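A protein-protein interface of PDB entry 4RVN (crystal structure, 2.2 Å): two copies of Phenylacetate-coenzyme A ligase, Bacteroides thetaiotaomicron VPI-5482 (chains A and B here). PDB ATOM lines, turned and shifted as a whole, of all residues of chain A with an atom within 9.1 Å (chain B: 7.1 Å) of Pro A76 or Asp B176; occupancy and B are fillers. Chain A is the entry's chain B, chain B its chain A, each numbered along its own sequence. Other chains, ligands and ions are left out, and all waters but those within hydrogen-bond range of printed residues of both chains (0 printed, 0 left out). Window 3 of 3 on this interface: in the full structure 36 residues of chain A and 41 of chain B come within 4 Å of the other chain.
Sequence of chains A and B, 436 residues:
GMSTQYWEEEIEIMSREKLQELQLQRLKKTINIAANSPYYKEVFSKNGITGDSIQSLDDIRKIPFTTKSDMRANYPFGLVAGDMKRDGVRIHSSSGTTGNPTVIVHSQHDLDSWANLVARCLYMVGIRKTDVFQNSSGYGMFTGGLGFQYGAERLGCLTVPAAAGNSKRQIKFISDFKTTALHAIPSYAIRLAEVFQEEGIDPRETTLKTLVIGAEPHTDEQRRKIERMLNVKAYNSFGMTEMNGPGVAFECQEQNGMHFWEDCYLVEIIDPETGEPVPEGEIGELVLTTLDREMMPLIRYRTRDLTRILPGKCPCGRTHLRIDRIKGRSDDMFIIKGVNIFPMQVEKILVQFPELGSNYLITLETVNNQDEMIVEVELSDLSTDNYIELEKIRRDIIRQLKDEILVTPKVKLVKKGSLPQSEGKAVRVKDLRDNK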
ATOM      1  N   ASP A  70       6.850   4.696   3.534  1.00  0.00           N
ATOM      2  CA  ASP A  70       7.876   5.659   3.962  1.00  0.00           C
ATOM      3  C   ASP A  70       8.557   5.185   5.247  1.00  0.00           C
ATOM      4  O   ASP A  70       9.777   5.307   5.385  1.00  0.00           O
ATOM      5  CB  ASP A  70       7.255   7.053   4.179  1.00  0.00           C
ATOM      6  CG  ASP A  70       6.739   7.733   2.925  1.00  0.00           C
ATOM      7  OD1 ASP A  70       7.411   7.634   1.877  1.00  0.00           O
ATOM      8  OD2 ASP A  70       5.721   8.455   3.018  1.00  0.00           O
ATOM      9  N   MET A  71       7.754   4.630   6.179  1.00  0.00           N
ATOM     10  CA  MET A  71       8.199   4.096   7.461  1.00  0.00           C
ATOM     11  C   MET A  71       8.993   2.815   7.249  1.00  0.00           C
ATOM     12  O   MET A  71      10.012   2.630   7.912  1.00  0.00           O
ATOM     13  CB  MET A  71       7.015   3.852   8.399  1.00  0.00           C
ATOM     14  CG  MET A  71       6.349   5.146   8.863  1.00  0.00           C
ATOM     15  SD  MET A  71       5.038   4.864  10.255  1.00  0.00           S
ATOM     16  CE  MET A  71       6.170   4.134  11.620  1.00  0.00           C
ATOM     17  N   ARG A  72       8.559   1.945   6.308  1.00  0.00           N
ATOM     18  CA  ARG A  72       9.303   0.714   5.998  1.00  0.00           C
ATOM     19  C   ARG A  72      10.664   1.042   5.376  1.00  0.00           C
ATOM     20  O   ARG A  72      11.650   0.365   5.671  1.00  0.00           O
ATOM     21  CB  ARG A  72       8.519  -0.218   5.055  1.00  0.00           C
ATOM     22  CG  ARG A  72       7.301  -0.892   5.678  1.00  0.00           C
ATOM     23  CD  ARG A  72       6.798  -1.991   4.768  1.00  0.00           C
ATOM     24  NE  ARG A  72       5.608  -2.658   5.297  1.00  0.00           N
ATOM     25  CZ  ARG A  72       4.379  -2.494   4.819  1.00  0.00           C
ATOM     26  NH1 ARG A  72       4.166  -1.706   3.771  1.00  0.00           N
ATOM     27  NH2 ARG A  72       3.358  -3.140   5.365  1.00  0.00           N
ATOM     28  N   ALA A  73      10.703   2.092   4.525  1.00  0.00           N
ATOM     29  CA  ALA A  73      11.895   2.569   3.831  1.00  0.00           C
ATOM     30  C   ALA A  73      12.912   3.182   4.801  1.00  0.00           C
ATOM     31  O   ALA A  73      14.109   3.166   4.507  1.00  0.00           O
ATOM     32  CB  ALA A  73      11.502   3.596   2.781  1.00  0.00           C
ATOM     33  N   ASN A  74      12.441   3.719   5.946  1.00  0.00           N
ATOM     34  CA  ASN A  74      13.308   4.350   6.936  1.00  0.00           C
ATOM     35  C   ASN A  74      13.397   3.513   8.227  1.00  0.00           C
ATOM     36  O   ASN A  74      13.776   4.043   9.279  1.00  0.00           O
ATOM     37  CB  ASN A  74      12.823   5.767   7.251  1.00  0.00           C
ATOM     38  CG  ASN A  74      13.062   6.744   6.128  1.00  0.00           C
ATOM     39  OD1 ASN A  74      14.035   7.510   6.138  1.00  0.00           O
ATOM     40  ND2 ASN A  74      12.196   6.725   5.125  1.00  0.00           N
ATOM     41  N   TYR A  75      13.113   2.200   8.130  1.00  0.00           N
ATOM     42  CA  TYR A  75      13.200   1.266   9.251  1.00  0.00           C
ATOM     43  C   TYR A  75      14.680   1.034   9.635  1.00  0.00           C
ATOM     44  O   TYR A  75      15.515   0.846   8.749  1.00  0.00           O
ATOM     45  CB  TYR A  75      12.505  -0.075   8.908  1.00  0.00           C
ATOM     46  CG  TYR A  75      12.696  -1.164   9.947  1.00  0.00           C
ATOM     47  CD1 TYR A  75      11.862  -1.249  11.060  1.00  0.00           C
ATOM     48  CD2 TYR A  75      13.710  -2.108   9.817  1.00  0.00           C
ATOM     49  CE1 TYR A  75      12.062  -2.223  12.042  1.00  0.00           C
ATOM     50  CE2 TYR A  75      13.914  -3.091  10.787  1.00  0.00           C
ATOM     51  CZ  TYR A  75      13.083  -3.149  11.895  1.00  0.00           C
ATOM     52  OH  TYR A  75      13.270  -4.123  12.846  1.00  0.00           O
ATOM     53  N   PRO A  76      15.031   1.059  10.939  1.00  0.00           N
ATOM     54  CA  PRO A  76      14.148   1.204  12.104  1.00  0.00           C
ATOM     55  C   PRO A  76      14.056   2.602  12.723  1.00  0.00           C
ATOM     56  O   PRO A  76      13.037   2.865  13.349  1.00  0.00           O
ATOM     57  CB  PRO A  76      14.799   0.273  13.138  1.00  0.00           C
ATOM     58  CG  PRO A  76      16.269   0.178  12.741  1.00  0.00           C
ATOM     59  CD  PRO A  76      16.418   0.767  11.353  1.00  0.00           C
ATOM     60  N   PHE A  77      15.080   3.469  12.613  1.00  0.00           N
ATOM     61  CA  PHE A  77      15.043   4.720  13.365  1.00  0.00           C
ATOM     62  C   PHE A  77      15.187   5.994  12.506  1.00  0.00           C
ATOM     63  O   PHE A  77      15.580   7.039  13.040  1.00  0.00           O
ATOM     64  CB  PHE A  77      16.178   4.707  14.410  1.00  0.00           C
ATOM     65  CG  PHE A  77      16.227   3.467  15.273  1.00  0.00           C
ATOM     66  CD1 PHE A  77      15.160   3.128  16.098  1.00  0.00           C
ATOM     67  CD2 PHE A  77      17.362   2.668  15.302  1.00  0.00           C
ATOM     68  CE1 PHE A  77      15.215   1.987  16.908  1.00  0.00           C
ATOM     69  CE2 PHE A  77      17.417   1.534  16.112  1.00  0.00           C
ATOM     70  CZ  PHE A  77      16.345   1.203  16.913  1.00  0.00           C
ATOM     71  N   GLY A  78      14.775   5.933  11.240  1.00  0.00           N
ATOM     72  CA  GLY A  78      14.812   7.086  10.341  1.00  0.00           C
ATOM     73  C   GLY A  78      13.917   8.254  10.740  1.00  0.00           C
ATOM     74  O   GLY A  78      14.195   9.396  10.375  1.00  0.00           O
ATOM     75  N   LEU A  79      12.848   7.986  11.513  1.00  0.00           N
ATOM     76  CA  LEU A  79      11.903   9.015  11.960  1.00  0.00           C
ATOM     77  C   LEU A  79      12.099   9.368  13.453  1.00  0.00           C
ATOM     78  O   LEU A  79      11.290  10.120  13.997  1.00  0.00           O
ATOM     79  CB  LEU A  79      10.442   8.585  11.715  1.00  0.00           C
ATOM     80  CG  LEU A  79       9.908   8.694  10.274  1.00  0.00           C
ATOM     81  CD1 LEU A  79      10.368   7.536   9.404  1.00  0.00           C
ATOM     82  CD2 LEU A  79       8.411   8.673  10.264  1.00  0.00           C
ATOM     83  N   VAL A  80      13.190   8.889  14.092  1.00  0.00           N
ATOM     84  CA  VAL A  80      13.482   9.203  15.499  1.00  0.00           C
ATOM     85  C   VAL A  80      14.030  10.639  15.539  1.00  0.00           C
ATOM     86  O   VAL A  80      15.045  10.935  14.904  1.00  0.00           O
ATOM     87  CB  VAL A  80      14.432   8.164  16.176  1.00  0.00           C
ATOM     88  CG1 VAL A  80      14.901   8.638  17.551  1.00  0.00           C
ATOM     89  CG2 VAL A  80      13.755   6.805  16.298  1.00  0.00           C
ATOM     90  N   MET A  84      17.636   9.230  21.493  1.00  0.00           N
ATOM     91  CA  MET A  84      17.247   7.863  21.809  1.00  0.00           C
ATOM     92  C   MET A  84      18.182   7.219  22.850  1.00  0.00           C
ATOM     93  O   MET A  84      17.687   6.566  23.770  1.00  0.00           O
ATOM     94  CB  MET A  84      17.241   7.043  20.512  1.00  0.00           C
ATOM     95  CG  MET A  84      16.665   5.656  20.670  1.00  0.00           C
ATOM     96  SD  MET A  84      16.456   4.718  18.979  1.00  0.00           S
ATOM     97  CE  MET A  84      18.258   4.712  18.319  1.00  0.00           C
ATOM     98  N   ILE A  91      10.756   0.494  22.896  1.00  0.00           N
ATOM     99  CA  ILE A  91      10.511   0.176  21.492  1.00  0.00           C
ATOM    100  C   ILE A  91       9.302  -0.769  21.408  1.00  0.00           C
ATOM    101  O   ILE A  91       9.317  -1.835  22.030  1.00  0.00           O
ATOM    102  CB  ILE A  91      11.763  -0.449  20.801  1.00  0.00           C
ATOM    103  CG1 ILE A  91      12.985   0.497  20.818  1.00  0.00           C
ATOM    104  CG2 ILE A  91      11.423  -0.904  19.374  1.00  0.00           C
ATOM    105  CD1 ILE A  91      14.303  -0.098  20.234  1.00  0.00           C
ATOM    106  N   HIS A  92       8.259  -0.386  20.659  1.00  0.00           N
ATOM    107  CA  HIS A  92       7.115  -1.251  20.378  1.00  0.00           C
ATOM    108  C   HIS A  92       7.099  -1.596  18.892  1.00  0.00           C
ATOM    109  O   HIS A  92       7.731  -0.892  18.108  1.00  0.00           O
ATOM    110  CB  HIS A  92       5.780  -0.621  20.805  1.00  0.00           C
ATOM    111  CG  HIS A  92       5.438  -0.847  22.244  1.00  0.00           C
ATOM    112  ND1 HIS A  92       5.008  -2.082  22.694  1.00  0.00           N
ATOM    113  CD2 HIS A  92       5.407   0.027  23.274  1.00  0.00           C
ATOM    114  CE1 HIS A  92       4.769  -1.933  23.985  1.00  0.00           C
ATOM    115  NE2 HIS A  92       4.988  -0.680  24.379  1.00  0.00           N
ATOM    116  N   GLY A  99       6.365  -8.996   6.419  1.00  0.00           N
ATOM    117  CA  GLY A  99       7.356  -8.037   5.941  1.00  0.00           C
ATOM    118  C   GLY A  99       8.239  -7.555   7.074  1.00  0.00           C
ATOM    119  O   GLY A  99       8.601  -8.347   7.952  1.00  0.00           O
ATOM    120  N   ASN A 100       8.589  -6.254   7.068  1.00  0.00           N
ATOM    121  CA  ASN A 100       9.395  -5.641   8.126  1.00  0.00           C
ATOM    122  C   ASN A 100       8.458  -4.859   9.061  1.00  0.00           C
ATOM    123  O   ASN A 100       7.918  -3.827   8.645  1.00  0.00           O
ATOM    124  CB  ASN A 100      10.510  -4.748   7.547  1.00  0.00           C
ATOM    125  CG  ASN A 100      11.923  -5.117   7.964  1.00  0.00           C
ATOM    126  OD1 ASN A 100      12.174  -6.104   8.665  1.00  0.00           O
ATOM    127  ND2 ASN A 100      12.890  -4.342   7.503  1.00  0.00           N
ATOM    128  N   PRO A 101       8.186  -5.361  10.294  1.00  0.00           N
ATOM    129  CA  PRO A 101       7.259  -4.644  11.192  1.00  0.00           C
ATOM    130  C   PRO A 101       7.773  -3.251  11.548  1.00  0.00           C
ATOM    131  O   PRO A 101       8.979  -3.057  11.700  1.00  0.00           O
ATOM    132  CB  PRO A 101       7.189  -5.545  12.435  1.00  0.00           C
ATOM    133  CG  PRO A 101       7.675  -6.878  11.979  1.00  0.00           C
ATOM    134  CD  PRO A 101       8.706  -6.585  10.938  1.00  0.00           C
ATOM    135  N   THR A 102       6.864  -2.273  11.632  1.00  0.00           N
ATOM    136  CA  THR A 102       7.253  -0.905  11.962  1.00  0.00           C
ATOM    137  C   THR A 102       7.500  -0.804  13.464  1.00  0.00           C
ATOM    138  O   THR A 102       6.880  -1.509  14.262  1.00  0.00           O
ATOM    139  CB  THR A 102       6.228   0.121  11.485  1.00  0.00           C
ATOM    140  OG1 THR A 102       4.944  -0.219  12.008  1.00  0.00           O
ATOM    141  CG2 THR A 102       6.191   0.245   9.958  1.00  0.00           C
ATOM    142  N   VAL A 103       8.429   0.071  13.827  1.00  0.00           N
ATOM    143  CA  VAL A 103       8.856   0.274  15.195  1.00  0.00           C
ATOM    144  C   VAL A 103       8.582   1.725  15.593  1.00  0.00           C
ATOM    145  O   VAL A 103       8.735   2.647  14.784  1.00  0.00           O
ATOM    146  CB  VAL A 103      10.354  -0.128  15.284  1.00  0.00           C
ATOM    147  CG1 VAL A 103      11.182   0.775  16.194  1.00  0.00           C
ATOM    148  CG2 VAL A 103      10.483  -1.595  15.661  1.00  0.00           C
ATOM    149  N   ILE A 104       8.108   1.893  16.841  1.00  0.00           N
ATOM    150  CA  ILE A 104       7.811   3.181  17.466  1.00  0.00           C
ATOM    151  C   ILE A 104       8.700   3.282  18.703  1.00  0.00           C
ATOM    152  O   ILE A 104       8.741   2.351  19.516  1.00  0.00           O
ATOM    153  CB  ILE A 104       6.291   3.354  17.780  1.00  0.00           C
ATOM    154  CG1 ILE A 104       5.391   3.151  16.521  1.00  0.00           C
ATOM    155  CG2 ILE A 104       5.990   4.689  18.487  1.00  0.00           C
ATOM    156  CD1 ILE A 104       5.604   4.133  15.301  1.00  0.00           C
ATOM    157  N   VAL A 105       9.446   4.388  18.818  1.00  0.00           N
ATOM    158  CA  VAL A 105      10.351   4.607  19.946  1.00  0.00           C
ATOM    159  C   VAL A 105       9.728   5.672  20.855  1.00  0.00           C
ATOM    160  O   VAL A 105       9.290   6.721  20.375  1.00  0.00           O
ATOM    161  CB  VAL A 105      11.783   4.980  19.487  1.00  0.00           C
ATOM    162  CG1 VAL A 105      12.748   4.999  20.670  1.00  0.00           C
ATOM    163  CG2 VAL A 105      12.284   4.001  18.431  1.00  0.00           C
ATOM    164  N   MET A 296       9.527  10.184  18.825  1.00  0.00           N
ATOM    165  CA  MET A 296       9.263   9.889  17.427  1.00  0.00           C
ATOM    166  C   MET A 296       7.839  10.359  17.061  1.00  0.00           C
ATOM    167  O   MET A 296       6.902   9.550  17.024  1.00  0.00           O
ATOM    168  CB  MET A 296       9.474   8.392  17.145  1.00  0.00           C
ATOM    169  CG  MET A 296       9.255   8.009  15.692  1.00  0.00           C
ATOM    170  SD  MET A 296       9.547   6.108  15.424  1.00  0.00           S
ATOM    171  CE  MET A 296       8.542   6.011  13.760  1.00  0.00           C
ATOM    172  N   ILE B 171      17.279 -12.273  17.607  1.00  0.00           N
ATOM    173  CA  ILE B 171      18.521 -11.974  16.880  1.00  0.00           C
ATOM    174  C   ILE B 171      18.295 -10.705  16.018  1.00  0.00           C
ATOM    175  O   ILE B 171      19.186  -9.856  15.949  1.00  0.00           O
ATOM    176  CB  ILE B 171      18.953 -13.231  16.034  1.00  0.00           C
ATOM    177  CG1 ILE B 171      19.883 -14.177  16.833  1.00  0.00           C
ATOM    178  CG2 ILE B 171      19.676 -12.870  14.728  1.00  0.00           C
ATOM    179  CD1 ILE B 171      19.379 -14.852  18.067  1.00  0.00           C
ATOM    180  N   LYS B 172      17.104 -10.573  15.397  1.00  0.00           N
ATOM    181  CA  LYS B 172      16.741  -9.414  14.573  1.00  0.00           C
ATOM    182  C   LYS B 172      16.720  -8.138  15.435  1.00  0.00           C
ATOM    183  O   LYS B 172      17.276  -7.123  15.013  1.00  0.00           O
ATOM    184  CB  LYS B 172      15.385  -9.626  13.874  1.00  0.00           C
ATOM    185  CG  LYS B 172      14.986  -8.457  12.977  1.00  0.00           C
ATOM    186  CD  LYS B 172      13.600  -8.595  12.352  1.00  0.00           C
ATOM    187  CE  LYS B 172      13.190  -7.343  11.622  1.00  0.00           C
ATOM    188  NZ  LYS B 172      14.107  -7.055  10.495  1.00  0.00           N
ATOM    189  N   PHE B 173      16.112  -8.201  16.639  1.00  0.00           N
ATOM    190  CA  PHE B 173      16.036  -7.066  17.564  1.00  0.00           C
ATOM    191  C   PHE B 173      17.433  -6.634  18.025  1.00  0.00           C
ATOM    192  O   PHE B 173      17.711  -5.435  18.040  1.00  0.00           O
ATOM    193  CB  PHE B 173      15.162  -7.384  18.790  1.00  0.00           C
ATOM    194  CG  PHE B 173      13.686  -7.642  18.571  1.00  0.00           C
ATOM    195  CD1 PHE B 173      13.033  -7.159  17.443  1.00  0.00           C
ATOM    196  CD2 PHE B 173      12.924  -8.266  19.548  1.00  0.00           C
ATOM    197  CE1 PHE B 173      11.658  -7.354  17.265  1.00  0.00           C
ATOM    198  CE2 PHE B 173      11.548  -8.462  19.368  1.00  0.00           C
ATOM    199  CZ  PHE B 173      10.923  -8.003  18.229  1.00  0.00           C
ATOM    200  N   ILE B 174      18.318  -7.604  18.351  1.00  0.00           N
ATOM    201  CA  ILE B 174      19.694  -7.345  18.793  1.00  0.00           C
ATOM    202  C   ILE B 174      20.473  -6.637  17.662  1.00  0.00           C
ATOM    203  O   ILE B 174      21.149  -5.645  17.928  1.00  0.00           O
ATOM    204  CB  ILE B 174      20.397  -8.663  19.252  1.00  0.00           C
ATOM    205  CG1 ILE B 174      19.735  -9.204  20.555  1.00  0.00           C
ATOM    206  CG2 ILE B 174      21.924  -8.461  19.453  1.00  0.00           C
ATOM    207  CD1 ILE B 174      20.081 -10.676  20.943  1.00  0.00           C
ATOM    208  N   SER B 175      20.344  -7.127  16.419  1.00  0.00           N
ATOM    209  CA  SER B 175      21.041  -6.597  15.246  1.00  0.00           C
ATOM    210  C   SER B 175      20.527  -5.203  14.828  1.00  0.00           C
ATOM    211  O   SER B 175      21.340  -4.335  14.513  1.00  0.00           O
ATOM    212  CB  SER B 175      20.895  -7.556  14.067  1.00  0.00           C
ATOM    213  OG  SER B 175      21.383  -8.851  14.384  1.00  0.00           O
ATOM    214  N   ASP B 176      19.197  -4.996  14.812  1.00  0.00           N
ATOM    215  CA  ASP B 176      18.581  -3.748  14.354  1.00  0.00           C
ATOM    216  C   ASP B 176      18.482  -2.662  15.441  1.00  0.00           C
ATOM    217  O   ASP B 176      18.586  -1.482  15.097  1.00  0.00           O
ATOM    218  CB  ASP B 176      17.163  -4.016  13.826  1.00  0.00           C
ATOM    219  CG  ASP B 176      17.051  -4.962  12.640  1.00  0.00           C
ATOM    220  OD1 ASP B 176      18.101  -5.329  12.065  1.00  0.00           O
ATOM    221  OD2 ASP B 176      15.912  -5.322  12.282  1.00  0.00           O
ATOM    222  N   PHE B 177      18.253  -3.028  16.720  1.00  0.00           N
ATOM    223  CA  PHE B 177      18.091  -2.009  17.766  1.00  0.00           C
ATOM    224  C   PHE B 177      19.400  -1.780  18.526  1.00  0.00           C
ATOM    225  O   PHE B 177      19.456  -0.892  19.379  1.00  0.00           O
ATOM    226  CB  PHE B 177      16.964  -2.381  18.751  1.00  0.00           C
ATOM    227  CG  PHE B 177      15.635  -2.761  18.127  1.00  0.00           C
ATOM    228  CD1 PHE B 177      15.192  -2.149  16.956  1.00  0.00           C
ATOM    229  CD2 PHE B 177      14.780  -3.652  18.763  1.00  0.00           C
ATOM    230  CE1 PHE B 177      13.966  -2.495  16.388  1.00  0.00           C
ATOM    231  CE2 PHE B 177      13.538  -3.970  18.209  1.00  0.00           C
ATOM    232  CZ  PHE B 177      13.150  -3.409  17.015  1.00  0.00           C
ATOM    233  N   LYS B 178      20.452  -2.552  18.183  1.00  0.00           N
ATOM    234  CA  LYS B 178      21.814  -2.519  18.743  1.00  0.00           C
ATOM    235  C   LYS B 178      21.759  -2.767  20.267  1.00  0.00           C
ATOM    236  O   LYS B 178      22.269  -1.966  21.058  1.00  0.00           O
ATOM    237  CB  LYS B 178      22.554  -1.196  18.411  1.00  0.00           C
ATOM    238  CG  LYS B 178      22.528  -0.765  16.938  1.00  0.00           C
ATOM    239  CD  LYS B 178      23.129  -1.780  15.971  1.00  0.00           C
ATOM    240  CE  LYS B 178      22.965  -1.338  14.539  1.00  0.00           C
ATOM    241  NZ  LYS B 178      23.448  -2.373  13.591  1.00  0.00           N
ATOM    242  N   THR B 179      21.137  -3.903  20.657  1.00  0.00           N
ATOM    243  CA  THR B 179      20.988  -4.360  22.046  1.00  0.00           C
ATOM    244  C   THR B 179      22.363  -4.572  22.671  1.00  0.00           C
ATOM    245  O   THR B 179      23.222  -5.204  22.058  1.00  0.00           O
ATOM    246  CB  THR B 179      20.155  -5.650  22.087  1.00  0.00           C
ATOM    247  OG1 THR B 179      18.878  -5.403  21.504  1.00  0.00           O
ATOM    248  CG2 THR B 179      19.988  -6.201  23.497  1.00  0.00           C
ATOM    249  N   THR B 207      26.502  -6.292  19.213  1.00  0.00           N
ATOM    250  CA  THR B 207      26.530  -5.109  20.079  1.00  0.00           C
ATOM    251  C   THR B 207      26.357  -5.506  21.562  1.00  0.00           C
ATOM    252  O   THR B 207      26.520  -4.650  22.432  1.00  0.00           O
ATOM    253  CB  THR B 207      25.439  -4.106  19.648  1.00  0.00           C
ATOM    254  OG1 THR B 207      24.181  -4.781  19.592  1.00  0.00           O
ATOM    255  CG2 THR B 207      25.735  -3.460  18.293  1.00  0.00           C
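No position is printed for both chains.
Of the 9 pairs that touch across the chains among the printed residues, none has its exchanged pair printed and touching as well.
Hydrophobic or aromatic side chains of chain A that line the printed part of chain B: Tyr A75, Pro A76, Phe A77, Ile A91 and Val A103.
Along chain B the printed residues that touch a printed residue of chain A span positions 172 to 177.
Among the printed residues, 9 pairs touch across the chains.
Among the printed residues, no Asp or Glu carboxylate lies within 4 Å of a Lys or Arg side-chain nitrogen of the other chain.
The side-chain carboxylate of Asp B176 is in salt-bridge range of the side-chain amino group of Lys B172 (3.1 Å).
Tyr A75 touches Lys B172.
Tyr A75 touches Phe B177.
Asp B176 touches Pro A76 (O to CG, 3.7 Å).
Asp B176 touches Phe A77.
Phe A77 touches Phe B177.
CG of Phe B177 touches CD1 of Ile A91, at 3.6 Å.
Val A103 touches Phe B177.
Of the printed residues of chain B, Pro A76 touches Asp B176.
Val A80 touches none of the printed residues of chain B.
Of the printed residues of chain A, Lys B172 touches Tyr A75 (3.4 Å) and Asn A100 (2.8 Å).
No residue of chain A comes within 4 Å of Ser B175.
Asp B176 touches just these residues of chain A: Tyr A75 (3.0 Å), Pro A76 (3.7 Å) and Phe A77 (3.4 Å).
Of the printed residues of chain A, Phe B177 touches Tyr A75, Phe A77, Ile A91 and Val A103.
Thr B207 touches none of the printed residues of chain A.
The nearest residue of chain B that does not touch Pro A76 is Phe B177 (4.3 Å).
The nearest residue of chain A that does not touch Asp B176 is Asn A100 (5.3 Å).
The nearest printed residue of chain B that does not touch Phe A77 is Lys B178 (5.5 Å).
NZ of Lys B172 is in hydrogen-bond range of OD1 of Asn A100 (2.8 Å).
OH of Tyr A75 is in hydrogen-bond range of OD2 of Asp B176, 3.0 Å away.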
